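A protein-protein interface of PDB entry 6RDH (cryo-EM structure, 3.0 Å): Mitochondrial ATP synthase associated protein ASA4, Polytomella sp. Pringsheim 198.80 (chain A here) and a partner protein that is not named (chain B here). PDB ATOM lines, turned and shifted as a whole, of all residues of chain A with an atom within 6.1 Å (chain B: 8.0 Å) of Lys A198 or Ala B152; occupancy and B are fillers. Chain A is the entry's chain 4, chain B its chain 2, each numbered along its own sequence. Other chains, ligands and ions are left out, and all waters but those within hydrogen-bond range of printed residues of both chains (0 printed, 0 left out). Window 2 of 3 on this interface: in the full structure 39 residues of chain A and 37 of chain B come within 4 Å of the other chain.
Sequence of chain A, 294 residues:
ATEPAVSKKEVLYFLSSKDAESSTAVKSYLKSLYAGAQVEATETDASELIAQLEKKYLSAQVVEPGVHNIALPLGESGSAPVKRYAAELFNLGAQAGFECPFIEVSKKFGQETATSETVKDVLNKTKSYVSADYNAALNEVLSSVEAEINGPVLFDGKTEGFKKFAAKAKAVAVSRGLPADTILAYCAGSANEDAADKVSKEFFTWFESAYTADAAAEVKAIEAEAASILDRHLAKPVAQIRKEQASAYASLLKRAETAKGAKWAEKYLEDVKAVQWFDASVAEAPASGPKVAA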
ATOM      1  N   GLU A 193      18.034  23.991 -16.810  1.00  0.00           N
ATOM      2  CA  GLU A 193      17.634  23.230 -15.633  1.00  0.00           C
ATOM      3  C   GLU A 193      16.126  23.249 -15.428  1.00  0.00           C
ATOM      4  O   GLU A 193      15.579  22.298 -14.864  1.00  0.00           O
ATOM      5  CB  GLU A 193      18.349  23.762 -14.385  1.00  0.00           C
ATOM      6  CG  GLU A 193      17.979  25.176 -13.980  1.00  0.00           C
ATOM      7  CD  GLU A 193      18.762  25.661 -12.781  1.00  0.00           C
ATOM      8  OE1 GLU A 193      19.186  26.834 -12.782  1.00  0.00           O
ATOM      9  OE2 GLU A 193      18.959  24.870 -11.838  1.00  0.00           O
ATOM     10  N   ASP A 194      15.441  24.274 -15.933  1.00  0.00           N
ATOM     11  CA  ASP A 194      13.995  24.377 -15.832  1.00  0.00           C
ATOM     12  C   ASP A 194      13.269  23.548 -16.880  1.00  0.00           C
ATOM     13  O   ASP A 194      12.037  23.565 -16.913  1.00  0.00           O
ATOM     14  CB  ASP A 194      13.571  25.841 -15.952  1.00  0.00           C
ATOM     15  CG  ASP A 194      14.120  26.696 -14.829  1.00  0.00           C
ATOM     16  OD1 ASP A 194      14.369  26.154 -13.733  1.00  0.00           O
ATOM     17  OD2 ASP A 194      14.303  27.912 -15.045  1.00  0.00           O
ATOM     18  N   ALA A 195      13.994  22.861 -17.758  1.00  0.00           N
ATOM     19  CA  ALA A 195      13.398  21.890 -18.661  1.00  0.00           C
ATOM     20  C   ALA A 195      14.048  20.524 -18.561  1.00  0.00           C
ATOM     21  O   ALA A 195      13.547  19.573 -19.167  1.00  0.00           O
ATOM     22  CB  ALA A 195      13.475  22.377 -20.111  1.00  0.00           C
ATOM     23  N   ALA A 196      15.158  20.408 -17.837  1.00  0.00           N
ATOM     24  CA  ALA A 196      15.681  19.107 -17.448  1.00  0.00           C
ATOM     25  C   ALA A 196      15.029  18.620 -16.168  1.00  0.00           C
ATOM     26  O   ALA A 196      14.741  17.429 -16.025  1.00  0.00           O
ATOM     27  CB  ALA A 196      17.197  19.173 -17.258  1.00  0.00           C
ATOM     28  N   ASP A 197      14.764  19.529 -15.237  1.00  0.00           N
ATOM     29  CA  ASP A 197      14.170  19.137 -13.973  1.00  0.00           C
ATOM     30  C   ASP A 197      12.672  18.899 -14.081  1.00  0.00           C
ATOM     31  O   ASP A 197      12.132  18.084 -13.326  1.00  0.00           O
ATOM     32  CB  ASP A 197      14.513  20.188 -12.925  1.00  0.00           C
ATOM     33  CG  ASP A 197      15.977  20.125 -12.524  1.00  0.00           C
ATOM     34  OD1 ASP A 197      16.524  19.004 -12.446  1.00  0.00           O
ATOM     35  OD2 ASP A 197      16.603  21.182 -12.335  1.00  0.00           O
ATOM     36  N   LYS A 198      12.003  19.521 -15.049  1.00  0.00           N
ATOM     37  CA  LYS A 198      10.603  19.203 -15.292  1.00  0.00           C
ATOM     38  C   LYS A 198      10.412  17.841 -15.937  1.00  0.00           C
ATOM     39  O   LYS A 198       9.287  17.332 -15.938  1.00  0.00           O
ATOM     40  CB  LYS A 198       9.957  20.279 -16.162  1.00  0.00           C
ATOM     41  CG  LYS A 198       9.794  21.646 -15.505  1.00  0.00           C
ATOM     42  CD  LYS A 198       8.592  21.718 -14.564  1.00  0.00           C
ATOM     43  CE  LYS A 198       8.962  21.624 -13.091  1.00  0.00           C
ATOM     44  NZ  LYS A 198       7.776  21.812 -12.210  1.00  0.00           N
ATOM     45  N   VAL A 199      11.463  17.238 -16.493  1.00  0.00           N
ATOM     46  CA  VAL A 199      11.366  15.851 -16.931  1.00  0.00           C
ATOM     47  C   VAL A 199      12.025  14.906 -15.927  1.00  0.00           C
ATOM     48  O   VAL A 199      11.713  13.706 -15.929  1.00  0.00           O
ATOM     49  CB  VAL A 199      11.949  15.645 -18.350  1.00  0.00           C
ATOM     50  CG1 VAL A 199      13.460  15.517 -18.338  1.00  0.00           C
ATOM     51  CG2 VAL A 199      11.283  14.471 -19.057  1.00  0.00           C
ATOM     52  N   SER A 200      12.886  15.413 -15.038  1.00  0.00           N
ATOM     53  CA  SER A 200      13.312  14.591 -13.910  1.00  0.00           C
ATOM     54  C   SER A 200      12.160  14.348 -12.950  1.00  0.00           C
ATOM     55  O   SER A 200      12.077  13.280 -12.345  1.00  0.00           O
ATOM     56  CB  SER A 200      14.460  15.238 -13.151  1.00  0.00           C
ATOM     57  OG  SER A 200      13.978  16.283 -12.335  1.00  0.00           O
ATOM     58  N   LYS A 201      11.252  15.315 -12.818  1.00  0.00           N
ATOM     59  CA  LYS A 201      10.057  15.103 -12.011  1.00  0.00           C
ATOM     60  C   LYS A 201       9.066  14.147 -12.657  1.00  0.00           C
ATOM     61  O   LYS A 201       8.150  13.689 -11.972  1.00  0.00           O
ATOM     62  CB  LYS A 201       9.359  16.427 -11.733  1.00  0.00           C
ATOM     63  CG  LYS A 201      10.108  17.321 -10.788  1.00  0.00           C
ATOM     64  CD  LYS A 201       9.574  18.716 -10.881  1.00  0.00           C
ATOM     65  CE  LYS A 201       8.195  18.799 -10.282  1.00  0.00           C
ATOM     66  NZ  LYS A 201       8.237  18.616  -8.807  1.00  0.00           N
ATOM     67  N   GLU A 202       9.193  13.864 -13.951  1.00  0.00           N
ATOM     68  CA  GLU A 202       8.402  12.804 -14.563  1.00  0.00           C
ATOM     69  C   GLU A 202       9.101  11.459 -14.493  1.00  0.00           C
ATOM     70  O   GLU A 202       8.438  10.422 -14.324  1.00  0.00           O
ATOM     71  CB  GLU A 202       8.102  13.125 -16.025  1.00  0.00           C
ATOM     72  CG  GLU A 202       7.218  14.324 -16.244  1.00  0.00           C
ATOM     73  CD  GLU A 202       6.954  14.567 -17.717  1.00  0.00           C
ATOM     74  OE1 GLU A 202       6.775  15.738 -18.111  1.00  0.00           O
ATOM     75  OE2 GLU A 202       6.928  13.582 -18.483  1.00  0.00           O
ATOM     76  N   ASN B 118       6.139  15.904  -5.087  1.00  0.00           N
ATOM     77  CA  ASN B 118       5.673  16.450  -6.359  1.00  0.00           C
ATOM     78  C   ASN B 118       4.326  17.142  -6.203  1.00  0.00           C
ATOM     79  O   ASN B 118       4.154  18.291  -6.633  1.00  0.00           O
ATOM     80  CB  ASN B 118       5.587  15.347  -7.411  1.00  0.00           C
ATOM     81  CG  ASN B 118       6.947  14.865  -7.860  1.00  0.00           C
ATOM     82  OD1 ASN B 118       7.071  13.805  -8.470  1.00  0.00           O
ATOM     83  ND2 ASN B 118       7.980  15.628  -7.538  1.00  0.00           N
ATOM     84  N   SER B 121       4.919  20.395  -4.029  1.00  0.00           N
ATOM     85  CA  SER B 121       5.569  21.480  -4.745  1.00  0.00           C
ATOM     86  C   SER B 121       4.663  22.062  -5.815  1.00  0.00           C
ATOM     87  O   SER B 121       4.677  23.280  -6.027  1.00  0.00           O
ATOM     88  CB  SER B 121       6.878  21.009  -5.356  1.00  0.00           C
ATOM     89  OG  SER B 121       7.877  20.883  -4.362  1.00  0.00           O
ATOM     90  N   ALA B 122       3.856  21.223  -6.475  1.00  0.00           N
ATOM     91  CA  ALA B 122       2.881  21.737  -7.432  1.00  0.00           C
ATOM     92  C   ALA B 122       1.831  22.608  -6.755  1.00  0.00           C
ATOM     93  O   ALA B 122       1.388  23.605  -7.334  1.00  0.00           O
ATOM     94  CB  ALA B 122       2.216  20.580  -8.169  1.00  0.00           C
ATOM     95  N   VAL B 124       2.384  24.377  -3.886  1.00  0.00           N
ATOM     96  CA  VAL B 124       2.963  25.607  -3.353  1.00  0.00           C
ATOM     97  C   VAL B 124       3.433  26.534  -4.481  1.00  0.00           C
ATOM     98  O   VAL B 124       3.575  27.745  -4.274  1.00  0.00           O
ATOM     99  CB  VAL B 124       4.086  25.269  -2.353  1.00  0.00           C
ATOM    100  CG1 VAL B 124       5.287  24.744  -3.062  1.00  0.00           C
ATOM    101  CG2 VAL B 124       4.437  26.453  -1.462  1.00  0.00           C
ATOM    102  N   VAL B 125       3.642  26.014  -5.700  1.00  0.00           N
ATOM    103  CA  VAL B 125       3.910  26.918  -6.820  1.00  0.00           C
ATOM    104  C   VAL B 125       2.675  27.213  -7.659  1.00  0.00           C
ATOM    105  O   VAL B 125       2.734  28.092  -8.532  1.00  0.00           O
ATOM    106  CB  VAL B 125       5.020  26.409  -7.759  1.00  0.00           C
ATOM    107  CG1 VAL B 125       6.249  26.018  -6.960  1.00  0.00           C
ATOM    108  CG2 VAL B 125       4.526  25.269  -8.635  1.00  0.00           C
ATOM    109  N   ILE B 128       1.131  30.554  -4.889  1.00  0.00           N
ATOM    110  CA  ILE B 128       2.274  30.998  -4.107  1.00  0.00           C
ATOM    111  C   ILE B 128       1.905  32.155  -3.179  1.00  0.00           C
ATOM    112  O   ILE B 128       2.574  32.373  -2.162  1.00  0.00           O
ATOM    113  CB  ILE B 128       3.431  31.343  -5.067  1.00  0.00           C
ATOM    114  CG1 ILE B 128       4.759  31.467  -4.326  1.00  0.00           C
ATOM    115  CG2 ILE B 128       3.140  32.614  -5.848  1.00  0.00           C
ATOM    116  CD1 ILE B 128       5.926  31.503  -5.236  1.00  0.00           C
ATOM    117  N   LEU B 140      10.422  24.113   1.450  1.00  0.00           N
ATOM    118  CA  LEU B 140      11.707  24.013   0.764  1.00  0.00           C
ATOM    119  C   LEU B 140      12.651  23.063   1.486  1.00  0.00           C
ATOM    120  O   LEU B 140      13.350  22.271   0.846  1.00  0.00           O
ATOM    121  CB  LEU B 140      12.330  25.401   0.650  1.00  0.00           C
ATOM    122  CG  LEU B 140      13.530  25.588  -0.267  1.00  0.00           C
ATOM    123  CD1 LEU B 140      13.088  25.643  -1.709  1.00  0.00           C
ATOM    124  CD2 LEU B 140      14.276  26.844   0.123  1.00  0.00           C
ATOM    125  N   ASN B 149      15.649  16.954  -6.303  1.00  0.00           N
ATOM    126  CA  ASN B 149      16.388  18.156  -6.676  1.00  0.00           C
ATOM    127  C   ASN B 149      15.468  19.138  -7.404  1.00  0.00           C
ATOM    128  O   ASN B 149      15.629  19.441  -8.583  1.00  0.00           O
ATOM    129  CB  ASN B 149      17.587  17.776  -7.531  1.00  0.00           C
ATOM    130  CG  ASN B 149      18.592  18.887  -7.645  1.00  0.00           C
ATOM    131  OD1 ASN B 149      18.588  19.643  -8.611  1.00  0.00           O
ATOM    132  ND2 ASN B 149      19.463  18.998  -6.655  1.00  0.00           N
ATOM    133  N   ASP B 150      14.477  19.626  -6.669  1.00  0.00           N
ATOM    134  CA  ASP B 150      13.438  20.472  -7.238  1.00  0.00           C
ATOM    135  C   ASP B 150      13.935  21.907  -7.273  1.00  0.00           C
ATOM    136  O   ASP B 150      14.060  22.554  -6.228  1.00  0.00           O
ATOM    137  CB  ASP B 150      12.151  20.363  -6.432  1.00  0.00           C
ATOM    138  CG  ASP B 150      10.932  20.490  -7.297  1.00  0.00           C
ATOM    139  OD1 ASP B 150       9.833  20.730  -6.764  1.00  0.00           O
ATOM    140  OD2 ASP B 150      11.083  20.357  -8.524  1.00  0.00           O
ATOM    141  N   VAL B 151      14.218  22.407  -8.479  1.00  0.00           N
ATOM    142  CA  VAL B 151      14.633  23.795  -8.634  1.00  0.00           C
ATOM    143  C   VAL B 151      13.478  24.705  -9.000  1.00  0.00           C
ATOM    144  O   VAL B 151      13.654  25.932  -9.006  1.00  0.00           O
ATOM    145  CB  VAL B 151      15.744  23.931  -9.689  1.00  0.00           C
ATOM    146  CG1 VAL B 151      16.816  22.877  -9.454  1.00  0.00           C
ATOM    147  CG2 VAL B 151      15.164  23.831 -11.081  1.00  0.00           C
ATOM    148  N   ALA B 152      12.301  24.153  -9.303  1.00  0.00           N
ATOM    149  CA  ALA B 152      11.125  24.988  -9.519  1.00  0.00           C
ATOM    150  C   ALA B 152      10.706  25.666  -8.223  1.00  0.00           C
ATOM    151  O   ALA B 152      10.528  26.890  -8.176  1.00  0.00           O
ATOM    152  CB  ALA B 152       9.985  24.150 -10.090  1.00  0.00           C
ATOM    153  N   LEU B 153      10.590  24.886  -7.148  1.00  0.00           N
ATOM    154  CA  LEU B 153      10.312  25.458  -5.839  1.00  0.00           C
ATOM    155  C   LEU B 153      11.486  26.287  -5.333  1.00  0.00           C
ATOM    156  O   LEU B 153      11.278  27.267  -4.615  1.00  0.00           O
ATOM    157  CB  LEU B 153       9.961  24.341  -4.855  1.00  0.00           C
ATOM    158  CG  LEU B 153       9.881  24.608  -3.347  1.00  0.00           C
ATOM    159  CD1 LEU B 153       8.870  25.686  -3.009  1.00  0.00           C
ATOM    160  CD2 LEU B 153       9.573  23.333  -2.596  1.00  0.00           C
ATOM    161  N   ALA B 154      12.711  25.952  -5.736  1.00  0.00           N
ATOM    162  CA  ALA B 154      13.859  26.755  -5.324  1.00  0.00           C
ATOM    163  C   ALA B 154      13.843  28.127  -5.985  1.00  0.00           C
ATOM    164  O   ALA B 154      14.163  29.135  -5.345  1.00  0.00           O
ATOM    165  CB  ALA B 154      15.153  26.016  -5.648  1.00  0.00           C
ATOM    166  N   LYS B 155      13.423  28.194  -7.251  1.00  0.00           N
ATOM    167  CA  LYS B 155      13.313  29.479  -7.932  1.00  0.00           C
ATOM    168  C   LYS B 155      12.130  30.285  -7.407  1.00  0.00           C
ATOM    169  O   LYS B 155      12.218  31.515  -7.275  1.00  0.00           O
ATOM    170  CB  LYS B 155      13.199  29.259  -9.439  1.00  0.00           C
ATOM    171  CG  LYS B 155      14.533  29.002 -10.116  1.00  0.00           C
ATOM    172  CD  LYS B 155      14.575  29.629 -11.490  1.00  0.00           C
ATOM    173  CE  LYS B 155      16.004  29.870 -11.949  1.00  0.00           C
ATOM    174  NZ  LYS B 155      16.066  30.769 -13.137  1.00  0.00           N
ATOM    175  N   ALA B 156      11.028  29.606  -7.076  1.00  0.00           N
ATOM    176  CA  ALA B 156       9.889  30.288  -6.467  1.00  0.00           C
ATOM    177  C   ALA B 156      10.228  30.848  -5.090  1.00  0.00           C
ATOM    178  O   ALA B 156       9.828  31.972  -4.755  1.00  0.00           O
ATOM    179  CB  ALA B 156       8.709  29.328  -6.370  1.00  0.00           C
ATOM    180  N   ALA B 157      10.988  30.096  -4.297  1.00  0.00           N
ATOM    181  CA  ALA B 157      11.443  30.584  -3.005  1.00  0.00           C
ATOM    182  C   ALA B 157      12.437  31.722  -3.157  1.00  0.00           C
ATOM    183  O   ALA B 157      12.428  32.649  -2.350  1.00  0.00           O
ATOM    184  CB  ALA B 157      12.062  29.448  -2.198  1.00  0.00           C
ATOM    185  N   GLY B 158      13.294  31.673  -4.182  1.00  0.00           N
ATOM    186  CA  GLY B 158      14.179  32.796  -4.447  1.00  0.00           C
ATOM    187  C   GLY B 158      13.439  34.074  -4.788  1.00  0.00           C
ATOM    188  O   GLY B 158      13.795  35.152  -4.297  1.00  0.00           O
ATOM    189  N   LYS B 159      12.364  33.958  -5.574  1.00  0.00           N
ATOM    190  CA  LYS B 159      11.539  35.121  -5.888  1.00  0.00           C
ATOM    191  C   LYS B 159      10.824  35.660  -4.653  1.00  0.00           C
ATOM    192  O   LYS B 159      10.768  36.880  -4.452  1.00  0.00           O
ATOM    193  CB  LYS B 159      10.540  34.759  -6.980  1.00  0.00           C
ATOM    194  CG  LYS B 159      11.197  34.649  -8.327  1.00  0.00           C
ATOM    195  CD  LYS B 159      10.327  33.954  -9.336  1.00  0.00           C
ATOM    196  CE  LYS B 159      11.058  33.866 -10.660  1.00  0.00           C
ATOM    197  NZ  LYS B 159      12.464  33.385 -10.498  1.00  0.00           N
ATOM    198  N   LEU B 181      20.524  21.191  -1.243  1.00  0.00           N
ATOM    199  CA  LEU B 181      20.290  21.156  -2.678  1.00  0.00           C
ATOM    200  C   LEU B 181      21.541  21.528  -3.464  1.00  0.00           C
ATOM    201  O   LEU B 181      21.703  21.090  -4.607  1.00  0.00           O
ATOM    202  CB  LEU B 181      19.139  22.087  -3.045  1.00  0.00           C
ATOM    203  CG  LEU B 181      17.764  21.438  -3.109  1.00  0.00           C
ATOM    204  CD1 LEU B 181      16.752  22.386  -3.707  1.00  0.00           C
ATOM    205  CD2 LEU B 181      17.828  20.166  -3.908  1.00  0.00           C
ATOM    206  N   ARG B 183      22.864  24.870  -4.393  1.00  0.00           N
ATOM    207  CA  ARG B 183      22.419  25.759  -5.456  1.00  0.00           C
ATOM    208  C   ARG B 183      23.167  27.080  -5.513  1.00  0.00           C
ATOM    209  O   ARG B 183      23.460  27.554  -6.614  1.00  0.00           O
ATOM    210  CB  ARG B 183      20.920  26.004  -5.317  1.00  0.00           C
ATOM    211  CG  ARG B 183      20.124  24.804  -5.758  1.00  0.00           C
ATOM    212  CD  ARG B 183      18.723  25.185  -6.117  1.00  0.00           C
ATOM    213  NE  ARG B 183      18.677  26.433  -6.863  1.00  0.00           N
ATOM    214  CZ  ARG B 183      18.832  26.524  -8.178  1.00  0.00           C
ATOM    215  NH1 ARG B 183      19.051  25.439  -8.904  1.00  0.00           N
ATOM    216  NH2 ARG B 183      18.768  27.706  -8.767  1.00  0.00           N
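The side-chain amide nitrogen of Asn B118 sits close to the side-chain amino group of Lys A201 (3.3 Å).
The side-chain amino group (NZ) of Lys A201 lies within salt-bridge range of the side-chain carboxylate (OD1) of Asp B150 (3.3 Å).
The side-chain amino group (NZ) of Lys B155 lies within salt-bridge range of the side-chain carboxylate (OD2) of Asp A194.
The guanidinium group (NH1) of Arg B183 is in salt-bridge range of the side-chain carboxylate (OE2) of Glu A193 (3.0 Å).
The side-chain carboxylate of Asp B150 is in hydrogen-bond range of the side-chain hydroxyl of Ser B121 (3.1 Å).
The backbone carbonyl oxygen of Asp A197 lies within hydrogen-bond range of the side-chain hydroxyl of Ser A200, at 2.8 Å.
Among the printed residues, merely in contact across the chains: Glu A193 with Val B151 (3.8 Å), Asp A194 with Val B151 (3.6 Å), Asp A197 with Asn B149 (3.99 Å), Asp A197 with Val B151 (3.3 Å) and Lys A198 with Ala B152 (3.9 Å).
Printed residues of chain A that touch a printed residue of chain B: Glu A193, Asp A194, Asp A197, Lys A198 and Lys A201.
Among the printed residues, 9 pairs touch across the chains.
Ala A196 touches none of the printed residues of chain B.
Of the printed residues of chain B, Asp A197 touches Asn B149 and Val B151.
Lys A198 touches one residue of chain B.
Printed residues of chain B within 4 Å of Lys A201: Asn B118 (3.3 Å) and Asp B150 (3.2 Å).
Glu A202 touches none of the printed residues of chain B.
Of the printed residues of chain A, Asn B118 touches Lys A201 (3.3 Å).
Of the printed residues of chain A, Asp B150 touches Lys A201.
Ala B152 touches just one residue of chain A: Lys A198 (3.9 Å).
Of the printed residues of chain A, Lys B155 touches Asp A194.
The nearest printed residue of chain A that does not touch Asp B150 is Lys A198 (5.2 Å).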
